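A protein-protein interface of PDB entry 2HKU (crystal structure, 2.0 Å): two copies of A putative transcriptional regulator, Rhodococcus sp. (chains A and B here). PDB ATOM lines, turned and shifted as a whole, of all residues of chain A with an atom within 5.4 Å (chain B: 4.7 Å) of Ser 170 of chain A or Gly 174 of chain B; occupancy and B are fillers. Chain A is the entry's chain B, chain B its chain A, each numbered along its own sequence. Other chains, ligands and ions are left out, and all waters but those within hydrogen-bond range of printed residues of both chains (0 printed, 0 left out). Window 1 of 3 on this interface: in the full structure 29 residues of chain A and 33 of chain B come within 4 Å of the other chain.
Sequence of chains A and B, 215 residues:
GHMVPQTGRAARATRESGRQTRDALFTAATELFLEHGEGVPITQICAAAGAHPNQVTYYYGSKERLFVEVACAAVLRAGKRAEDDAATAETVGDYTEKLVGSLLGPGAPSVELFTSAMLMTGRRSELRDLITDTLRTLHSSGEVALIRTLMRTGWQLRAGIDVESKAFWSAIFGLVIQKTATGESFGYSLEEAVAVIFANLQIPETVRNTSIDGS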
ATOM      1  N   SER A 165       6.521   7.482  26.404  1.00  0.00           N
ATOM      2  CA  SER A 165       7.817   8.057  26.488  1.00  0.00           C
ATOM      3  C   SER A 165       8.824   7.062  25.887  1.00  0.00           C
ATOM      4  O   SER A 165       9.712   7.445  25.128  1.00  0.00           O
ATOM      5  CB  SER A 165       8.162   8.523  27.939  1.00  0.00           C
ATOM      6  OG  SER A 165       9.361   9.282  27.968  1.00  0.00           O
ATOM      7  N   LYS A 166       8.668   5.774  26.121  1.00  0.00           N
ATOM      8  CA  LYS A 166       9.591   4.827  25.537  1.00  0.00           C
ATOM      9  C   LYS A 166       9.412   4.801  24.055  1.00  0.00           C
ATOM     10  O   LYS A 166      10.345   4.558  23.384  1.00  0.00           O
ATOM     11  CB  LYS A 166       9.313   3.412  26.100  1.00  0.00           C
ATOM     12  CG  LYS A 166       9.745   3.204  27.597  1.00  0.00           C
ATOM     13  CD  LYS A 166       9.244   1.742  27.922  1.00  0.00           C
ATOM     14  CE  LYS A 166       9.027   1.508  29.390  1.00  0.00           C
ATOM     15  NZ  LYS A 166       8.307   0.203  29.618  1.00  0.00           N
ATOM     16  N   ALA A 167       8.188   4.976  23.562  1.00  0.00           N
ATOM     17  CA  ALA A 167       7.926   4.871  22.125  1.00  0.00           C
ATOM     18  C   ALA A 167       8.544   6.116  21.440  1.00  0.00           C
ATOM     19  O   ALA A 167       9.189   6.020  20.384  1.00  0.00           O
ATOM     20  CB  ALA A 167       6.403   4.809  21.871  1.00  0.00           C
ATOM     21  N   PHE A 168       8.505   7.237  22.144  1.00  0.00           N
ATOM     22  CA  PHE A 168       9.120   8.488  21.615  1.00  0.00           C
ATOM     23  C   PHE A 168      10.615   8.302  21.485  1.00  0.00           C
ATOM     24  O   PHE A 168      11.156   8.435  20.388  1.00  0.00           O
ATOM     25  CB  PHE A 168       8.794   9.709  22.510  1.00  0.00           C
ATOM     26  CG  PHE A 168       9.575  10.957  22.095  1.00  0.00           C
ATOM     27  CD1 PHE A 168       9.143  11.693  21.016  1.00  0.00           C
ATOM     28  CD2 PHE A 168      10.818  11.263  22.688  1.00  0.00           C
ATOM     29  CE1 PHE A 168       9.848  12.844  20.585  1.00  0.00           C
ATOM     30  CE2 PHE A 168      11.617  12.505  22.235  1.00  0.00           C
ATOM     31  CZ  PHE A 168      11.068  13.206  21.167  1.00  0.00           C
ATOM     32  N   TRP A 169      11.292   7.901  22.572  1.00  0.00           N
ATOM     33  CA  TRP A 169      12.742   7.793  22.550  1.00  0.00           C
ATOM     34  C   TRP A 169      13.242   6.669  21.675  1.00  0.00           C
ATOM     35  O   TRP A 169      14.245   6.847  21.026  1.00  0.00           O
ATOM     36  CB  TRP A 169      13.336   7.664  23.977  1.00  0.00           C
ATOM     37  CG  TRP A 169      13.248   8.928  24.662  1.00  0.00           C
ATOM     38  CD1 TRP A 169      12.406   9.286  25.681  1.00  0.00           C
ATOM     39  CD2 TRP A 169      13.974  10.119  24.291  1.00  0.00           C
ATOM     40  NE1 TRP A 169      12.628  10.637  26.028  1.00  0.00           N
ATOM     41  CE2 TRP A 169      13.589  11.153  25.201  1.00  0.00           C
ATOM     42  CE3 TRP A 169      14.991  10.369  23.357  1.00  0.00           C
ATOM     43  CZ2 TRP A 169      14.143  12.455  25.144  1.00  0.00           C
ATOM     44  CZ3 TRP A 169      15.552  11.702  23.307  1.00  0.00           C
ATOM     45  CH2 TRP A 169      15.139  12.666  24.187  1.00  0.00           C
ATOM     46  N   SER A 170      12.586   5.473  21.718  1.00  0.00           N
ATOM     47  CA  SER A 170      12.938   4.425  20.769  1.00  0.00           C
ATOM     48  C   SER A 170      12.841   4.927  19.307  1.00  0.00           C
ATOM     49  O   SER A 170      13.718   4.620  18.506  1.00  0.00           O
ATOM     50  CB  SER A 170      12.057   3.180  20.969  1.00  0.00           C
ATOM     51  OG  SER A 170      12.149   2.662  22.328  1.00  0.00           O
ATOM     52  N   ALA A 171      11.777   5.631  18.962  1.00  0.00           N
ATOM     53  CA  ALA A 171      11.705   6.223  17.610  1.00  0.00           C
ATOM     54  C   ALA A 171      12.872   7.112  17.367  1.00  0.00           C
ATOM     55  O   ALA A 171      13.520   6.956  16.340  1.00  0.00           O
ATOM     56  CB  ALA A 171      10.330   6.972  17.322  1.00  0.00           C
ATOM     57  N   ILE A 172      13.123   8.081  18.276  1.00  0.00           N
ATOM     58  CA  ILE A 172      14.186   9.037  18.078  1.00  0.00           C
ATOM     59  C   ILE A 172      15.577   8.370  17.897  1.00  0.00           C
ATOM     60  O   ILE A 172      16.311   8.703  16.955  1.00  0.00           O
ATOM     61  CB  ILE A 172      14.263  10.132  19.244  1.00  0.00           C
ATOM     62  CG1 ILE A 172      13.038  11.065  19.240  1.00  0.00           C
ATOM     63  CG2 ILE A 172      15.693  10.870  19.284  1.00  0.00           C
ATOM     64  CD1 ILE A 172      12.788  11.900  17.932  1.00  0.00           C
ATOM     65  N   PHE A 173      15.967   7.427  18.759  1.00  0.00           N
ATOM     66  CA  PHE A 173      17.255   6.714  18.611  1.00  0.00           C
ATOM     67  C   PHE A 173      17.314   5.927  17.301  1.00  0.00           C
ATOM     68  O   PHE A 173      18.306   5.935  16.597  1.00  0.00           O
ATOM     69  CB  PHE A 173      17.485   5.783  19.795  1.00  0.00           C
ATOM     70  CG  PHE A 173      17.648   6.528  21.112  1.00  0.00           C
ATOM     71  CD1 PHE A 173      18.502   7.604  21.220  1.00  0.00           C
ATOM     72  CD2 PHE A 173      16.963   6.125  22.231  1.00  0.00           C
ATOM     73  CE1 PHE A 173      18.631   8.308  22.452  1.00  0.00           C
ATOM     74  CE2 PHE A 173      17.143   6.751  23.427  1.00  0.00           C
ATOM     75  CZ  PHE A 173      17.931   7.846  23.555  1.00  0.00           C
ATOM     76  N   GLY A 174      16.210   5.317  16.929  1.00  0.00           N
ATOM     77  CA  GLY A 174      16.136   4.525  15.701  1.00  0.00           C
ATOM     78  C   GLY A 174      16.158   5.327  14.408  1.00  0.00           C
ATOM     79  O   GLY A 174      16.657   4.812  13.380  1.00  0.00           O
ATOM     80  N   LEU A 175      15.717   6.577  14.479  1.00  0.00           N
ATOM     81  CA  LEU A 175      15.705   7.511  13.334  1.00  0.00           C
ATOM     82  C   LEU A 175      17.052   8.227  13.184  1.00  0.00           C
ATOM     83  O   LEU A 175      17.611   8.360  12.048  1.00  0.00           O
ATOM     84  CB  LEU A 175      14.596   8.575  13.530  1.00  0.00           C
ATOM     85  CG  LEU A 175      13.161   8.121  13.207  1.00  0.00           C
ATOM     86  CD1 LEU A 175      12.183   9.051  13.790  1.00  0.00           C
ATOM     87  CD2 LEU A 175      12.915   7.903  11.747  1.00  0.00           C
ATOM     88  N   SER B 170      12.249   1.838  12.881  1.00  0.00           N
ATOM     89  CA  SER B 170      13.008   2.701  13.832  1.00  0.00           C
ATOM     90  C   SER B 170      12.711   2.422  15.297  1.00  0.00           C
ATOM     91  O   SER B 170      13.612   2.483  16.103  1.00  0.00           O
ATOM     92  CB  SER B 170      12.733   4.151  13.559  1.00  0.00           C
ATOM     93  OG  SER B 170      11.348   4.333  13.535  1.00  0.00           O
ATOM     94  N   ALA B 171      11.463   2.032  15.616  1.00  0.00           N
ATOM     95  CA  ALA B 171      11.117   1.433  16.972  1.00  0.00           C
ATOM     96  C   ALA B 171      11.949   0.164  17.287  1.00  0.00           C
ATOM     97  O   ALA B 171      12.547   0.009  18.374  1.00  0.00           O
ATOM     98  CB  ALA B 171       9.577   1.095  17.069  1.00  0.00           C
ATOM     99  N   ILE B 172      11.935  -0.792  16.341  1.00  0.00           N
ATOM    100  CA  ILE B 172      12.754  -1.951  16.511  1.00  0.00           C
ATOM    101  C   ILE B 172      14.230  -1.596  16.829  1.00  0.00           C
ATOM    102  O   ILE B 172      14.764  -2.096  17.794  1.00  0.00           O
ATOM    103  CB  ILE B 172      12.624  -2.981  15.318  1.00  0.00           C
ATOM    104  CG1 ILE B 172      11.177  -3.579  15.252  1.00  0.00           C
ATOM    105  CG2 ILE B 172      13.715  -4.015  15.421  1.00  0.00           C
ATOM    106  CD1 ILE B 172      10.814  -4.590  16.400  1.00  0.00           C
ATOM    107  N   PHE B 173      14.861  -0.743  16.009  1.00  0.00           N
ATOM    108  CA  PHE B 173      16.255  -0.289  16.246  1.00  0.00           C
ATOM    109  C   PHE B 173      16.442   0.319  17.630  1.00  0.00           C
ATOM    110  O   PHE B 173      17.322  -0.110  18.403  1.00  0.00           O
ATOM    111  CB  PHE B 173      16.696   0.723  15.159  1.00  0.00           C
ATOM    112  CG  PHE B 173      16.694   0.154  13.742  1.00  0.00           C
ATOM    113  CD1 PHE B 173      17.034  -1.175  13.498  1.00  0.00           C
ATOM    114  CD2 PHE B 173      16.364   0.972  12.670  1.00  0.00           C
ATOM    115  CE1 PHE B 173      17.012  -1.659  12.129  1.00  0.00           C
ATOM    116  CE2 PHE B 173      16.348   0.534  11.330  1.00  0.00           C
ATOM    117  CZ  PHE B 173      16.641  -0.737  11.069  1.00  0.00           C
ATOM    118  N   GLY B 174      15.567   1.246  17.977  1.00  0.00           N
ATOM    119  CA  GLY B 174      15.662   1.973  19.314  1.00  0.00           C
ATOM    120  C   GLY B 174      15.365   1.042  20.503  1.00  0.00           C
ATOM    121  O   GLY B 174      15.968   1.165  21.593  1.00  0.00           O
ATOM    122  N   LEU B 175      14.432   0.109  20.322  1.00  0.00           N
ATOM    123  CA  LEU B 175      14.184  -0.904  21.377  1.00  0.00           C
ATOM    124  C   LEU B 175      15.337  -1.885  21.549  1.00  0.00           C
ATOM    125  O   LEU B 175      15.736  -2.185  22.682  1.00  0.00           O
ATOM    126  CB  LEU B 175      12.878  -1.701  21.161  1.00  0.00           C
ATOM    127  CG  LEU B 175      11.670  -0.842  21.211  1.00  0.00           C
ATOM    128  CD1 LEU B 175      10.390  -1.336  20.440  1.00  0.00           C
ATOM    129  CD2 LEU B 175      11.381  -0.489  22.647  1.00  0.00           C
ATOM    130  N   VAL B 176      15.888  -2.375  20.464  1.00  0.00           N
ATOM    131  CA  VAL B 176      17.073  -3.255  20.539  1.00  0.00           C
ATOM    132  C   VAL B 176      18.241  -2.554  21.192  1.00  0.00           C
ATOM    133  O   VAL B 176      18.920  -3.149  21.990  1.00  0.00           O
ATOM    134  CB  VAL B 176      17.560  -3.834  19.154  1.00  0.00           C
ATOM    135  CG1 VAL B 176      18.948  -4.517  19.256  1.00  0.00           C
ATOM    136  CG2 VAL B 176      16.524  -4.860  18.644  1.00  0.00           C
ATOM    137  N   ILE B 177      18.504  -1.314  20.815  1.00  0.00           N
ATOM    138  CA  ILE B 177      19.639  -0.620  21.376  1.00  0.00           C
ATOM    139  C   ILE B 177      19.489  -0.440  22.908  1.00  0.00           C
ATOM    140  O   ILE B 177      20.413  -0.725  23.675  1.00  0.00           O
ATOM    141  CB  ILE B 177      19.799   0.791  20.695  1.00  0.00           C
ATOM    142  CG1 ILE B 177      20.294   0.569  19.245  1.00  0.00           C
ATOM    143  CG2 ILE B 177      20.875   1.533  21.463  1.00  0.00           C
ATOM    144  CD1 ILE B 177      20.032   1.755  18.247  1.00  0.00           C
ATOM    145  N   GLN B 178      18.354   0.042  23.354  1.00  0.00           N
ATOM    146  CA  GLN B 178      18.143   0.338  24.764  1.00  0.00           C
ATOM    147  C   GLN B 178      17.991  -0.895  25.590  1.00  0.00           C
ATOM    148  O   GLN B 178      18.334  -0.953  26.780  1.00  0.00           O
ATOM    149  CB  GLN B 178      16.866   1.089  24.908  1.00  0.00           C
ATOM    150  CG  GLN B 178      17.089   2.571  24.369  1.00  0.00           C
ATOM    151  CD  GLN B 178      15.873   3.336  24.438  1.00  0.00           C
ATOM    152  OE1 GLN B 178      15.702   4.225  25.328  1.00  0.00           O
ATOM    153  NE2 GLN B 178      14.979   3.099  23.500  1.00  0.00           N
ATOM    154  N   TYR B 188      13.018  -1.721  29.710  1.00  0.00           N
ATOM    155  CA  TYR B 188      13.270  -2.321  28.401  1.00  0.00           C
ATOM    156  C   TYR B 188      13.574  -3.791  28.532  1.00  0.00           C
ATOM    157  O   TYR B 188      14.514  -4.274  27.895  1.00  0.00           O
ATOM    158  CB  TYR B 188      14.379  -1.585  27.591  1.00  0.00           C
ATOM    159  CG  TYR B 188      13.899  -0.231  27.054  1.00  0.00           C
ATOM    160  CD1 TYR B 188      13.091  -0.158  25.939  1.00  0.00           C
ATOM    161  CD2 TYR B 188      14.186   0.964  27.733  1.00  0.00           C
ATOM    162  CE1 TYR B 188      12.565   1.111  25.441  1.00  0.00           C
ATOM    163  CE2 TYR B 188      13.703   2.252  27.211  1.00  0.00           C
ATOM    164  CZ  TYR B 188      12.900   2.299  26.057  1.00  0.00           C
ATOM    165  OH  TYR B 188      12.440   3.552  25.547  1.00  0.00           O
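Ser 170 of chain B touches its own counterpart, Ser 170 of chain A.
Ser 170 of chain A touches Gly 174 of chain B, and with the chains exchanged Gly 174 of chain A touches Ser 170 of chain B.
Ser 170 of chain A touches Leu 175 of chain B, and with the chains exchanged Leu 175 of chain A touches Ser 170 of chain B.
Gly 174 of chain A touches Phe 173 of chain B, but with the chains exchanged Phe 173 of chain A does not touch Gly 174 of chain B (4.3 Å).
Positions printed for both chains: 170, 171, 172, 173, 174 and 175.
Of the 10 pairs that touch across the chains among the printed residues, 5 have their exchanged pair printed and touching as well.
The side-chain hydroxyl (OH) of Tyr 188 of chain B sits at hydrogen-bond distance from the side-chain amide nitrogen (NE2) of Gln 178 of chain B (3.3 Å).
The backbone carbonyl oxygen of Lys 166 of chain A is in hydrogen-bond range of the side-chain hydroxyl of Ser 170 of chain A, at 2.8 Å.
The side-chain amide nitrogen (NE2) of Gln 178 of chain B lies within hydrogen-bond range of the backbone carbonyl oxygen (O) of Gly 174 of chain B, 2.9 Å away.
NE2 of Gln 178 of chain B lies within hydrogen-bond range of OG of Ser 170 of chain A (3.1 Å).
The backbone carbonyl oxygen of Ser 170 of chain A lies close to the backbone carbonyl oxygen of Ser 170 of chain B, 3.2 Å away.
OH of Tyr 188 of chain B lies within hydrogen-bond range of OG of Ser 170 of chain A.
The side-chain hydroxyl of Tyr 188 of chain B sits close to the backbone carbonyl oxygen of Lys 166 of chain A (3.2 Å).
Gly 174 of chain B touches Ser 170 of chain A (CA to O, 3.4 Å).
Ser 170 of chain A touches Leu 175 of chain B (OG to CD2, 3.3 Å).
CE2 of Phe 173 of chain A touches OE1 of Gln 178 of chain B, at 3.5 Å.
Ser 170 of chain B touches Gly 174 of chain A (O to CA, 3.3 Å).
Gly 174 of chain A touches Phe 173 of chain B (CA to CB, 3.9 Å).
N of Leu 175 of chain A touches CB of Ser 170 of chain B, at 3.95 Å.
Printed residues of chain B within 4 Å of Lys 166 of chain A: Tyr 188 (3.1 Å).
Of chain B, only Ser 170 (3.2 Å), Gly 174 (3.4 Å), Leu 175 (3.3 Å), Gln 178 (3.1 Å) and Tyr 188 (3.4 Å) come within 4 Å of Ser 170 of chain A.
Ile 172 of chain A touches none of the printed residues of chain B.
Of the printed residues of chain A, Tyr 188 of chain B touches Lys 166 and Ser 170.
The nearest residue of chain A that does not touch Gly 174 of chain B is Gly 174 of chain A (4.03 Å).
The nearest printed residue of chain A that does not touch Gln 178 of chain B is Trp 169 of chain A (4.4 Å).
Of the 11 printed residues of chain A, 5 touch a printed residue of chain B.
Printed residues of chain B that touch a printed residue of chain A: Ser 170, Phe 173, Gly 174, Leu 175, Gln 178 and Tyr 188.
Hydrophobic or aromatic side chains of chain B that line the printed part of chain A: Phe 173, Leu 175 and Tyr 188.
Among the printed residues, 10 pairs touch across the chains.
Among the printed residues, no Asp or Glu carboxylate lies within 4 Å of a Lys or Arg side-chain nitrogen of the other chain.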
